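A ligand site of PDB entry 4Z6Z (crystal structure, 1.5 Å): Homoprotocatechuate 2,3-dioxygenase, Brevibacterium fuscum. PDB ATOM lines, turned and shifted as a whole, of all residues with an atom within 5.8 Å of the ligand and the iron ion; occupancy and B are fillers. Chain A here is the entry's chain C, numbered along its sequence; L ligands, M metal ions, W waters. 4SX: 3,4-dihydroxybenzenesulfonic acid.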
ATOM      1  N   HIS A 155      14.670   9.614 -31.217  1.00  0.00           N
ATOM      2  CA  HIS A 155      14.619   8.359 -30.447  1.00  0.00           C
ATOM      3  C   HIS A 155      13.999   8.535 -29.085  1.00  0.00           C
ATOM      4  O   HIS A 155      13.841   9.662 -28.584  1.00  0.00           O
ATOM      5  CB  HIS A 155      16.016   7.701 -30.314  1.00  0.00           C
ATOM      6  CG  HIS A 155      17.029   8.509 -29.560  1.00  0.00           C
ATOM      7  ND1 HIS A 155      17.955   9.333 -30.178  1.00  0.00           N
ATOM      8  CD2 HIS A 155      17.310   8.568 -28.239  1.00  0.00           C
ATOM      9  CE1 HIS A 155      18.739   9.878 -29.266  1.00  0.00           C
ATOM     10  NE2 HIS A 155      18.362   9.428 -28.075  1.00  0.00           N
ATOM     11  N   PHE A 156      13.731   7.384 -28.464  1.00  0.00           N
ATOM     12  CA  PHE A 156      13.462   7.284 -27.050  1.00  0.00           C
ATOM     13  C   PHE A 156      14.598   6.559 -26.328  1.00  0.00           C
ATOM     14  O   PHE A 156      15.387   5.830 -26.946  1.00  0.00           O
ATOM     15  CB  PHE A 156      12.187   6.483 -26.817  1.00  0.00           C
ATOM     16  CG  PHE A 156      11.017   6.871 -27.679  1.00  0.00           C
ATOM     17  CD1 PHE A 156      10.495   8.160 -27.646  1.00  0.00           C
ATOM     18  CD2 PHE A 156      10.382   5.934 -28.496  1.00  0.00           C
ATOM     19  CE1 PHE A 156       9.385   8.492 -28.418  1.00  0.00           C
ATOM     20  CE2 PHE A 156       9.275   6.258 -29.246  1.00  0.00           C
ATOM     21  CZ  PHE A 156       8.784   7.549 -29.225  1.00  0.00           C
ATOM     22  N   ASN A 157      14.668   6.714 -25.021  1.00  0.00           N
ATOM     23  CA  ASN A 157      15.588   5.934 -24.201  1.00  0.00           C
ATOM     24  C   ASN A 157      14.857   5.497 -22.923  1.00  0.00           C
ATOM     25  O   ASN A 157      14.259   6.308 -22.223  1.00  0.00           O
ATOM     26  CB  ASN A 157      16.854   6.731 -23.906  1.00  0.00           C
ATOM     27  CG  ASN A 157      17.891   5.929 -23.146  1.00  0.00           C
ATOM     28  OD1 ASN A 157      17.621   5.412 -22.074  1.00  0.00           O
ATOM     29  ND2 ASN A 157      19.079   5.828 -23.711  1.00  0.00           N
ATOM     30  N   ILE A 181      27.243  -1.147 -24.261  1.00  0.00           N
ATOM     31  CA  ILE A 181      28.268  -0.962 -23.237  1.00  0.00           C
ATOM     32  C   ILE A 181      28.244  -2.197 -22.331  1.00  0.00           C
ATOM     33  O   ILE A 181      27.189  -2.562 -21.807  1.00  0.00           O
ATOM     34  CB  ILE A 181      27.997   0.291 -22.360  1.00  0.00           C
ATOM     35  CG1 ILE A 181      28.047   1.580 -23.193  1.00  0.00           C
ATOM     36  CG2 ILE A 181      28.985   0.354 -21.210  1.00  0.00           C
ATOM     37  CD1 ILE A 181      27.636   2.840 -22.434  1.00  0.00           C
ATOM     38  N   TRP A 192      21.691   0.106 -27.721  1.00  0.00           N
ATOM     39  CA  TRP A 192      21.031   1.034 -28.654  1.00  0.00           C
ATOM     40  C   TRP A 192      20.550   0.240 -29.849  1.00  0.00           C
ATOM     41  O   TRP A 192      21.258  -0.615 -30.357  1.00  0.00           O
ATOM     42  CB  TRP A 192      22.028   2.095 -29.132  1.00  0.00           C
ATOM     43  CG  TRP A 192      22.351   3.161 -28.124  1.00  0.00           C
ATOM     44  CD1 TRP A 192      21.924   4.453 -28.156  1.00  0.00           C
ATOM     45  CD2 TRP A 192      23.200   3.049 -26.962  1.00  0.00           C
ATOM     46  NE1 TRP A 192      22.425   5.149 -27.076  1.00  0.00           N
ATOM     47  CE2 TRP A 192      23.211   4.318 -26.331  1.00  0.00           C
ATOM     48  CE3 TRP A 192      23.978   2.015 -26.408  1.00  0.00           C
ATOM     49  CZ2 TRP A 192      23.947   4.569 -25.179  1.00  0.00           C
ATOM     50  CZ3 TRP A 192      24.694   2.283 -25.238  1.00  0.00           C
ATOM     51  CH2 TRP A 192      24.686   3.551 -24.644  1.00  0.00           C
ATOM     52  N   HIS A 200      19.757   4.748 -33.458  1.00  0.00           N
ATOM     53  CA  HIS A 200      18.622   4.168 -32.713  1.00  0.00           C
ATOM     54  C   HIS A 200      17.288   4.816 -32.911  1.00  0.00           C
ATOM     55  O   HIS A 200      17.193   5.981 -33.267  1.00  0.00           O
ATOM     56  CB  HIS A 200      18.922   4.015 -31.215  1.00  0.00           C
ATOM     57  CG  HIS A 200      19.294   5.257 -30.482  1.00  0.00           C
ATOM     58  ND1 HIS A 200      20.143   6.225 -30.974  1.00  0.00           N
ATOM     59  CD2 HIS A 200      18.992   5.632 -29.215  1.00  0.00           C
ATOM     60  CE1 HIS A 200      20.354   7.133 -30.041  1.00  0.00           C
ATOM     61  NE2 HIS A 200      19.672   6.798 -28.964  1.00  0.00           N
ATOM     62  N   HIS A 214      14.699   9.557 -21.530  1.00  0.00           N
ATOM     63  CA  HIS A 214      14.552  10.791 -22.320  1.00  0.00           C
ATOM     64  C   HIS A 214      13.843  10.557 -23.637  1.00  0.00           C
ATOM     65  O   HIS A 214      13.682   9.412 -24.094  1.00  0.00           O
ATOM     66  CB  HIS A 214      15.894  11.508 -22.524  1.00  0.00           C
ATOM     67  CG  HIS A 214      16.933  10.731 -23.274  1.00  0.00           C
ATOM     68  ND1 HIS A 214      17.892   9.984 -22.642  1.00  0.00           N
ATOM     69  CD2 HIS A 214      17.195  10.637 -24.594  1.00  0.00           C
ATOM     70  CE1 HIS A 214      18.712   9.455 -23.531  1.00  0.00           C
ATOM     71  NE2 HIS A 214      18.294   9.820 -24.720  1.00  0.00           N
ATOM     72  N   ALA A 216      14.452  12.254 -27.535  1.00  0.00           N
ATOM     73  CA  ALA A 216      15.492  13.011 -28.265  1.00  0.00           C
ATOM     74  C   ALA A 216      14.953  13.574 -29.574  1.00  0.00           C
ATOM     75  O   ALA A 216      14.319  12.866 -30.362  1.00  0.00           O
ATOM     76  CB  ALA A 216      16.687  12.125 -28.555  1.00  0.00           C
ATOM     77  N   ARG A 243      23.237  18.020 -18.525  1.00  0.00           N
ATOM     78  CA  ARG A 243      24.468  17.364 -18.997  1.00  0.00           C
ATOM     79  C   ARG A 243      24.760  17.817 -20.431  1.00  0.00           C
ATOM     80  O   ARG A 243      23.871  17.903 -21.235  1.00  0.00           O
ATOM     81  CB  ARG A 243      24.326  15.847 -18.951  1.00  0.00           C
ATOM     82  CG  ARG A 243      25.465  15.079 -19.602  1.00  0.00           C
ATOM     83  CD  ARG A 243      25.389  13.560 -19.429  1.00  0.00           C
ATOM     84  NE  ARG A 243      26.392  12.989 -20.343  1.00  0.00           N
ATOM     85  CZ  ARG A 243      26.262  11.916 -21.122  1.00  0.00           C
ATOM     86  NH1 ARG A 243      25.227  11.078 -21.052  1.00  0.00           N
ATOM     87  NH2 ARG A 243      27.236  11.627 -21.965  1.00  0.00           N
ATOM     88  N   HIS A 248      29.070  12.483 -27.985  1.00  0.00           N
ATOM     89  CA  HIS A 248      28.942  11.127 -27.457  1.00  0.00           C
ATOM     90  C   HIS A 248      30.063  10.221 -27.986  1.00  0.00           C
ATOM     91  O   HIS A 248      30.544  10.399 -29.115  1.00  0.00           O
ATOM     92  CB  HIS A 248      27.613  10.496 -27.870  1.00  0.00           C
ATOM     93  CG  HIS A 248      26.409  10.959 -27.122  1.00  0.00           C
ATOM     94  ND1 HIS A 248      26.329  10.948 -25.741  1.00  0.00           N
ATOM     95  CD2 HIS A 248      25.189  11.340 -27.565  1.00  0.00           C
ATOM     96  CE1 HIS A 248      25.117  11.332 -25.370  1.00  0.00           C
ATOM     97  NE2 HIS A 248      24.410  11.574 -26.458  1.00  0.00           N
ATOM     98  N   GLY A 249      30.443   9.235 -27.202  1.00  0.00           N
ATOM     99  CA  GLY A 249      31.229   8.114 -27.729  1.00  0.00           C
ATOM    100  C   GLY A 249      30.327   7.197 -28.518  1.00  0.00           C
ATOM    101  O   GLY A 249      30.313   7.171 -29.759  1.00  0.00           O
ATOM    102  N   VAL A 250      29.513   6.442 -27.793  1.00  0.00           N
ATOM    103  CA  VAL A 250      28.406   5.743 -28.396  1.00  0.00           C
ATOM    104  C   VAL A 250      27.580   6.703 -29.266  1.00  0.00           C
ATOM    105  O   VAL A 250      27.137   7.745 -28.783  1.00  0.00           O
ATOM    106  CB  VAL A 250      27.494   5.152 -27.290  1.00  0.00           C
ATOM    107  CG1 VAL A 250      26.238   4.553 -27.931  1.00  0.00           C
ATOM    108  CG2 VAL A 250      28.238   4.123 -26.460  1.00  0.00           C
ATOM    109  N   SER A 251      27.377   6.345 -30.530  1.00  0.00           N
ATOM    110  CA  SER A 251      26.601   7.093 -31.550  1.00  0.00           C
ATOM    111  C   SER A 251      27.373   8.164 -32.296  1.00  0.00           C
ATOM    112  O   SER A 251      26.960   8.528 -33.385  1.00  0.00           O
ATOM    113  CB  SER A 251      25.289   7.700 -31.027  1.00  0.00           C
ATOM    114  OG  SER A 251      25.501   8.938 -30.370  1.00  0.00           O
ATOM    115  N   TYR A 255      25.479  16.383 -28.596  1.00  0.00           N
ATOM    116  CA  TYR A 255      24.290  16.209 -27.712  1.00  0.00           C
ATOM    117  C   TYR A 255      24.198  17.271 -26.620  1.00  0.00           C
ATOM    118  O   TYR A 255      25.188  17.918 -26.262  1.00  0.00           O
ATOM    119  CB  TYR A 255      24.312  14.834 -27.049  1.00  0.00           C
ATOM    120  CG  TYR A 255      25.351  14.695 -25.956  1.00  0.00           C
ATOM    121  CD1 TYR A 255      25.057  15.081 -24.668  1.00  0.00           C
ATOM    122  CD2 TYR A 255      26.629  14.227 -26.220  1.00  0.00           C
ATOM    123  CE1 TYR A 255      25.990  14.986 -23.666  1.00  0.00           C
ATOM    124  CE2 TYR A 255      27.595  14.115 -25.207  1.00  0.00           C
ATOM    125  CZ  TYR A 255      27.265  14.497 -23.928  1.00  0.00           C
ATOM    126  OH  TYR A 255      28.195  14.394 -22.911  1.00  0.00           O
ATOM    127  N   TYR A 257      21.498  17.514 -22.847  1.00  0.00           N
ATOM    128  CA  TYR A 257      20.315  17.101 -22.076  1.00  0.00           C
ATOM    129  C   TYR A 257      19.795  18.231 -21.210  1.00  0.00           C
ATOM    130  O   TYR A 257      20.555  18.838 -20.442  1.00  0.00           O
ATOM    131  CB  TYR A 257      20.588  15.904 -21.167  1.00  0.00           C
ATOM    132  CG  TYR A 257      21.081  14.672 -21.888  1.00  0.00           C
ATOM    133  CD1 TYR A 257      20.188  13.720 -22.401  1.00  0.00           C
ATOM    134  CD2 TYR A 257      22.432  14.483 -22.087  1.00  0.00           C
ATOM    135  CE1 TYR A 257      20.659  12.592 -23.057  1.00  0.00           C
ATOM    136  CE2 TYR A 257      22.909  13.354 -22.736  1.00  0.00           C
ATOM    137  CZ  TYR A 257      22.026  12.422 -23.229  1.00  0.00           C
ATOM    138  OH  TYR A 257      22.502  11.295 -23.864  1.00  0.00           O
ATOM    139  N   GLU A 267      16.661  15.191 -24.832  1.00  0.00           N
ATOM    140  CA  GLU A 267      17.977  15.262 -25.451  1.00  0.00           C
ATOM    141  C   GLU A 267      17.851  15.992 -26.778  1.00  0.00           C
ATOM    142  O   GLU A 267      16.870  15.807 -27.513  1.00  0.00           O
ATOM    143  CB  GLU A 267      18.570  13.862 -25.708  1.00  0.00           C
ATOM    144  CG  GLU A 267      20.001  13.897 -26.243  1.00  0.00           C
ATOM    145  CD  GLU A 267      20.563  12.541 -26.537  1.00  0.00           C
ATOM    146  OE1 GLU A 267      19.776  11.569 -26.540  1.00  0.00           O
ATOM    147  OE2 GLU A 267      21.773  12.431 -26.756  1.00  0.00           O
ATOM    148  N   TYR A 269      20.204  16.346 -30.270  1.00  0.00           N
ATOM    149  CA  TYR A 269      21.100  15.322 -30.830  1.00  0.00           C
ATOM    150  C   TYR A 269      21.348  15.647 -32.301  1.00  0.00           C
ATOM    151  O   TYR A 269      20.449  16.096 -32.993  1.00  0.00           O
ATOM    152  CB  TYR A 269      20.361  13.999 -30.651  1.00  0.00           C
ATOM    153  CG  TYR A 269      20.968  12.707 -31.120  1.00  0.00           C
ATOM    154  CD1 TYR A 269      21.660  11.882 -30.218  1.00  0.00           C
ATOM    155  CD2 TYR A 269      20.735  12.230 -32.407  1.00  0.00           C
ATOM    156  CE1 TYR A 269      22.145  10.635 -30.609  1.00  0.00           C
ATOM    157  CE2 TYR A 269      21.235  10.980 -32.796  1.00  0.00           C
ATOM    158  CZ  TYR A 269      21.927  10.196 -31.893  1.00  0.00           C
ATOM    159  OH  TYR A 269      22.406   8.951 -32.277  1.00  0.00           O
ATOM    160  N   ARG A 292      33.398   6.801 -23.481  1.00  0.00           N
ATOM    161  CA  ARG A 292      32.264   6.078 -24.076  1.00  0.00           C
ATOM    162  C   ARG A 292      30.973   6.895 -24.142  1.00  0.00           C
ATOM    163  O   ARG A 292      30.176   6.714 -25.042  1.00  0.00           O
ATOM    164  CB  ARG A 292      32.006   4.764 -23.320  1.00  0.00           C
ATOM    165  CG  ARG A 292      31.250   4.953 -22.013  1.00  0.00           C
ATOM    166  CD  ARG A 292      31.347   3.781 -21.034  1.00  0.00           C
ATOM    167  NE  ARG A 292      30.614   4.182 -19.822  1.00  0.00           N
ATOM    168  CZ  ARG A 292      31.080   5.024 -18.884  1.00  0.00           C
ATOM    169  NH1 ARG A 292      32.299   5.525 -18.949  1.00  0.00           N
ATOM    170  NH2 ARG A 292      30.310   5.372 -17.855  1.00  0.00           N
ATOM    171  N   ARG A 293      30.759   7.748 -23.133  1.00  0.00           N
ATOM    172  CA  ARG A 293      29.530   8.518 -23.031  1.00  0.00           C
ATOM    173  C   ARG A 293      29.759   9.968 -23.442  1.00  0.00           C
ATOM    174  O   ARG A 293      28.969  10.550 -24.214  1.00  0.00           O
ATOM    175  CB  ARG A 293      28.933   8.407 -21.619  1.00  0.00           C
ATOM    176  CG  ARG A 293      28.305   7.026 -21.368  1.00  0.00           C
ATOM    177  CD  ARG A 293      27.152   7.070 -20.393  1.00  0.00           C
ATOM    178  NE  ARG A 293      26.482   5.789 -20.164  1.00  0.00           N
ATOM    179  CZ  ARG A 293      25.373   5.356 -20.785  1.00  0.00           C
ATOM    180  NH1 ARG A 293      24.776   6.052 -21.736  1.00  0.00           N
ATOM    181  NH2 ARG A 293      24.835   4.185 -20.410  1.00  0.00           N
ATOM    182  N   ASP A 294      30.810  10.568 -22.917  1.00  0.00           N
ATOM    183  CA  ASP A 294      31.303  11.837 -23.428  1.00  0.00           C
ATOM    184  C   ASP A 294      32.727  11.597 -23.952  1.00  0.00           C
ATOM    185  O   ASP A 294      33.621  11.227 -23.198  1.00  0.00           O
ATOM    186  CB  ASP A 294      31.302  12.907 -22.359  1.00  0.00           C
ATOM    187  CG  ASP A 294      31.603  14.272 -22.940  1.00  0.00           C
ATOM    188  OD1 ASP A 294      30.641  14.944 -23.406  1.00  0.00           O
ATOM    189  OD2 ASP A 294      32.794  14.675 -22.923  1.00  0.00           O
ATOM    190  N   TRP A 304      21.971  11.960 -14.049  1.00  0.00           N
ATOM    191  CA  TRP A 304      21.744  11.355 -15.363  1.00  0.00           C
ATOM    192  C   TRP A 304      21.560   9.843 -15.256  1.00  0.00           C
ATOM    193  O   TRP A 304      20.758   9.260 -15.986  1.00  0.00           O
ATOM    194  CB  TRP A 304      22.876  11.737 -16.341  1.00  0.00           C
ATOM    195  CG  TRP A 304      22.528  11.517 -17.761  1.00  0.00           C
ATOM    196  CD1 TRP A 304      21.931  12.411 -18.592  1.00  0.00           C
ATOM    197  CD2 TRP A 304      22.690  10.322 -18.517  1.00  0.00           C
ATOM    198  NE1 TRP A 304      21.751  11.867 -19.825  1.00  0.00           N
ATOM    199  CE2 TRP A 304      22.217  10.574 -19.811  1.00  0.00           C
ATOM    200  CE3 TRP A 304      23.228   9.052 -18.237  1.00  0.00           C
ATOM    201  CZ2 TRP A 304      22.228   9.622 -20.815  1.00  0.00           C
ATOM    202  CZ3 TRP A 304      23.233   8.102 -19.235  1.00  0.00           C
ATOM    203  CH2 TRP A 304      22.743   8.391 -20.513  1.00  0.00           C
HETATM  204  O11 4SX L   1      26.075   9.198 -23.275  1.00  0.00           O
HETATM  205  S9  4SX L   1      26.095   8.073 -24.429  1.00  0.00           S
HETATM  206  O12 4SX L   1      27.257   8.280 -25.340  1.00  0.00           O
HETATM  207  O10 4SX L   1      26.183   6.751 -23.818  1.00  0.00           O
HETATM  208  C4  4SX L   1      24.642   8.114 -25.354  1.00  0.00           C
HETATM  209  C3  4SX L   1      23.458   8.521 -24.705  1.00  0.00           C
HETATM  210  C5  4SX L   1      24.688   7.985 -26.756  1.00  0.00           C
HETATM  211  C6  4SX L   1      23.560   8.288 -27.555  1.00  0.00           C
HETATM  212  C1  4SX L   1      22.406   8.770 -26.912  1.00  0.00           C
HETATM  213  O7  4SX L   1      21.324   9.213 -27.660  1.00  0.00           O
HETATM  214  C2  4SX L   1      22.356   8.892 -25.481  1.00  0.00           C
HETATM  215  O8  4SX L   1      21.252   9.378 -24.893  1.00  0.00           O
HETATM  216 FE    FE M   1      19.735   9.563 -26.340  1.00  0.00          FE
HETATM  217  O   HOH W   1      19.599   7.200 -26.205  1.00  0.00           O
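The side-chain hydroxyl (OH) of Tyr 257 lies close to an oxygen (O8) of the ligand, 2.5 Å away.
O of Arg 293 lies close to O12 of the ligand (3.1 Å).
O10 of the ligand is in salt-bridge range of NH1 of Arg 293, 2.6 Å away.
A ring nitrogen (ND1) of His 248 sits at hydrogen-bond distance from an oxygen (O12) of the ligand (2.9 Å).
NH2 of Arg 243 lies within salt-bridge range of O11 of the ligand, at 3.0 Å.
A ring nitrogen (NE2) of His 200 sits close to an oxygen (O7) of the ligand.
OH of Tyr 257 is in hydrogen-bond range of OE2 of Glu 267, at 3.2 Å.
The backbone carbonyl oxygen (O) of His 214 sits at hydrogen-bond distance from the backbone NH (N) of Asn 157, at 3.0 Å.
O of His 155 lies within hydrogen-bond range of N of Ala 216, at 2.9 Å.
The backbone carbonyl oxygen (O) of Arg 243 lies within hydrogen-bond range of the backbone NH (N) of Tyr 257, at 2.9 Å.
The backbone carbonyl oxygen of Arg 293 is in hydrogen-bond range of a ring nitrogen (ND1) of His 248 (3.1 Å).
The backbone carbonyl oxygen (O) of Arg 293 sits at hydrogen-bond distance from the guanidinium group (NH2) of Arg 243 (3.0 Å).
The backbone carbonyl oxygen of Arg 292 is in hydrogen-bond range of the backbone NH of Val 250 (2.8 Å).
The backbone NH (N) of Gly 249 lies close to the backbone carbonyl oxygen (O) of Arg 292.
An oxygen (O12) of the ligand sits close to the backbone carbonyl oxygen of Val 250, 3.5 Å away.
An oxygen (O12) of the ligand lies close to the backbone carbonyl oxygen (O) of Arg 292 (3.3 Å).
Trp 192 touches the ligand.
N of Gly 249 touches O12 of the ligand, at 3.8 Å.
Ser 251 touches the ligand (OG to C6, 3.5 Å).
Tyr 269 touches the ligand.
Hydrophobic or aromatic side chains that line the ligand: His 155, Trp 192, His 200, His 214, His 248, Val 250, Tyr 257 and Tyr 269.
The nearest printed residue that does not touch the ligand is Trp 304 (4.2 Å).
His 200 touches the iron ion.
Of the 21 residues printed, 4 come within 4 Å of the iron ion.
The nearest printed residue that does not touch the iron ion is Tyr 257 (4.1 Å).
The iron ion is bound by OE1 of Glu 267 (2.0 Å), O7 of the ligand (2.1 Å), O8 of the ligand (2.1 Å), NE2 of His 214 (2.2 Å), NE2 of His 155 (2.2 Å) and water W1 (2.4 Å).
Water W1 lies within hydrogen-bond range of NE2 of His 200 (2.8 Å) and ND2 of Asn 157 (2.9 Å).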
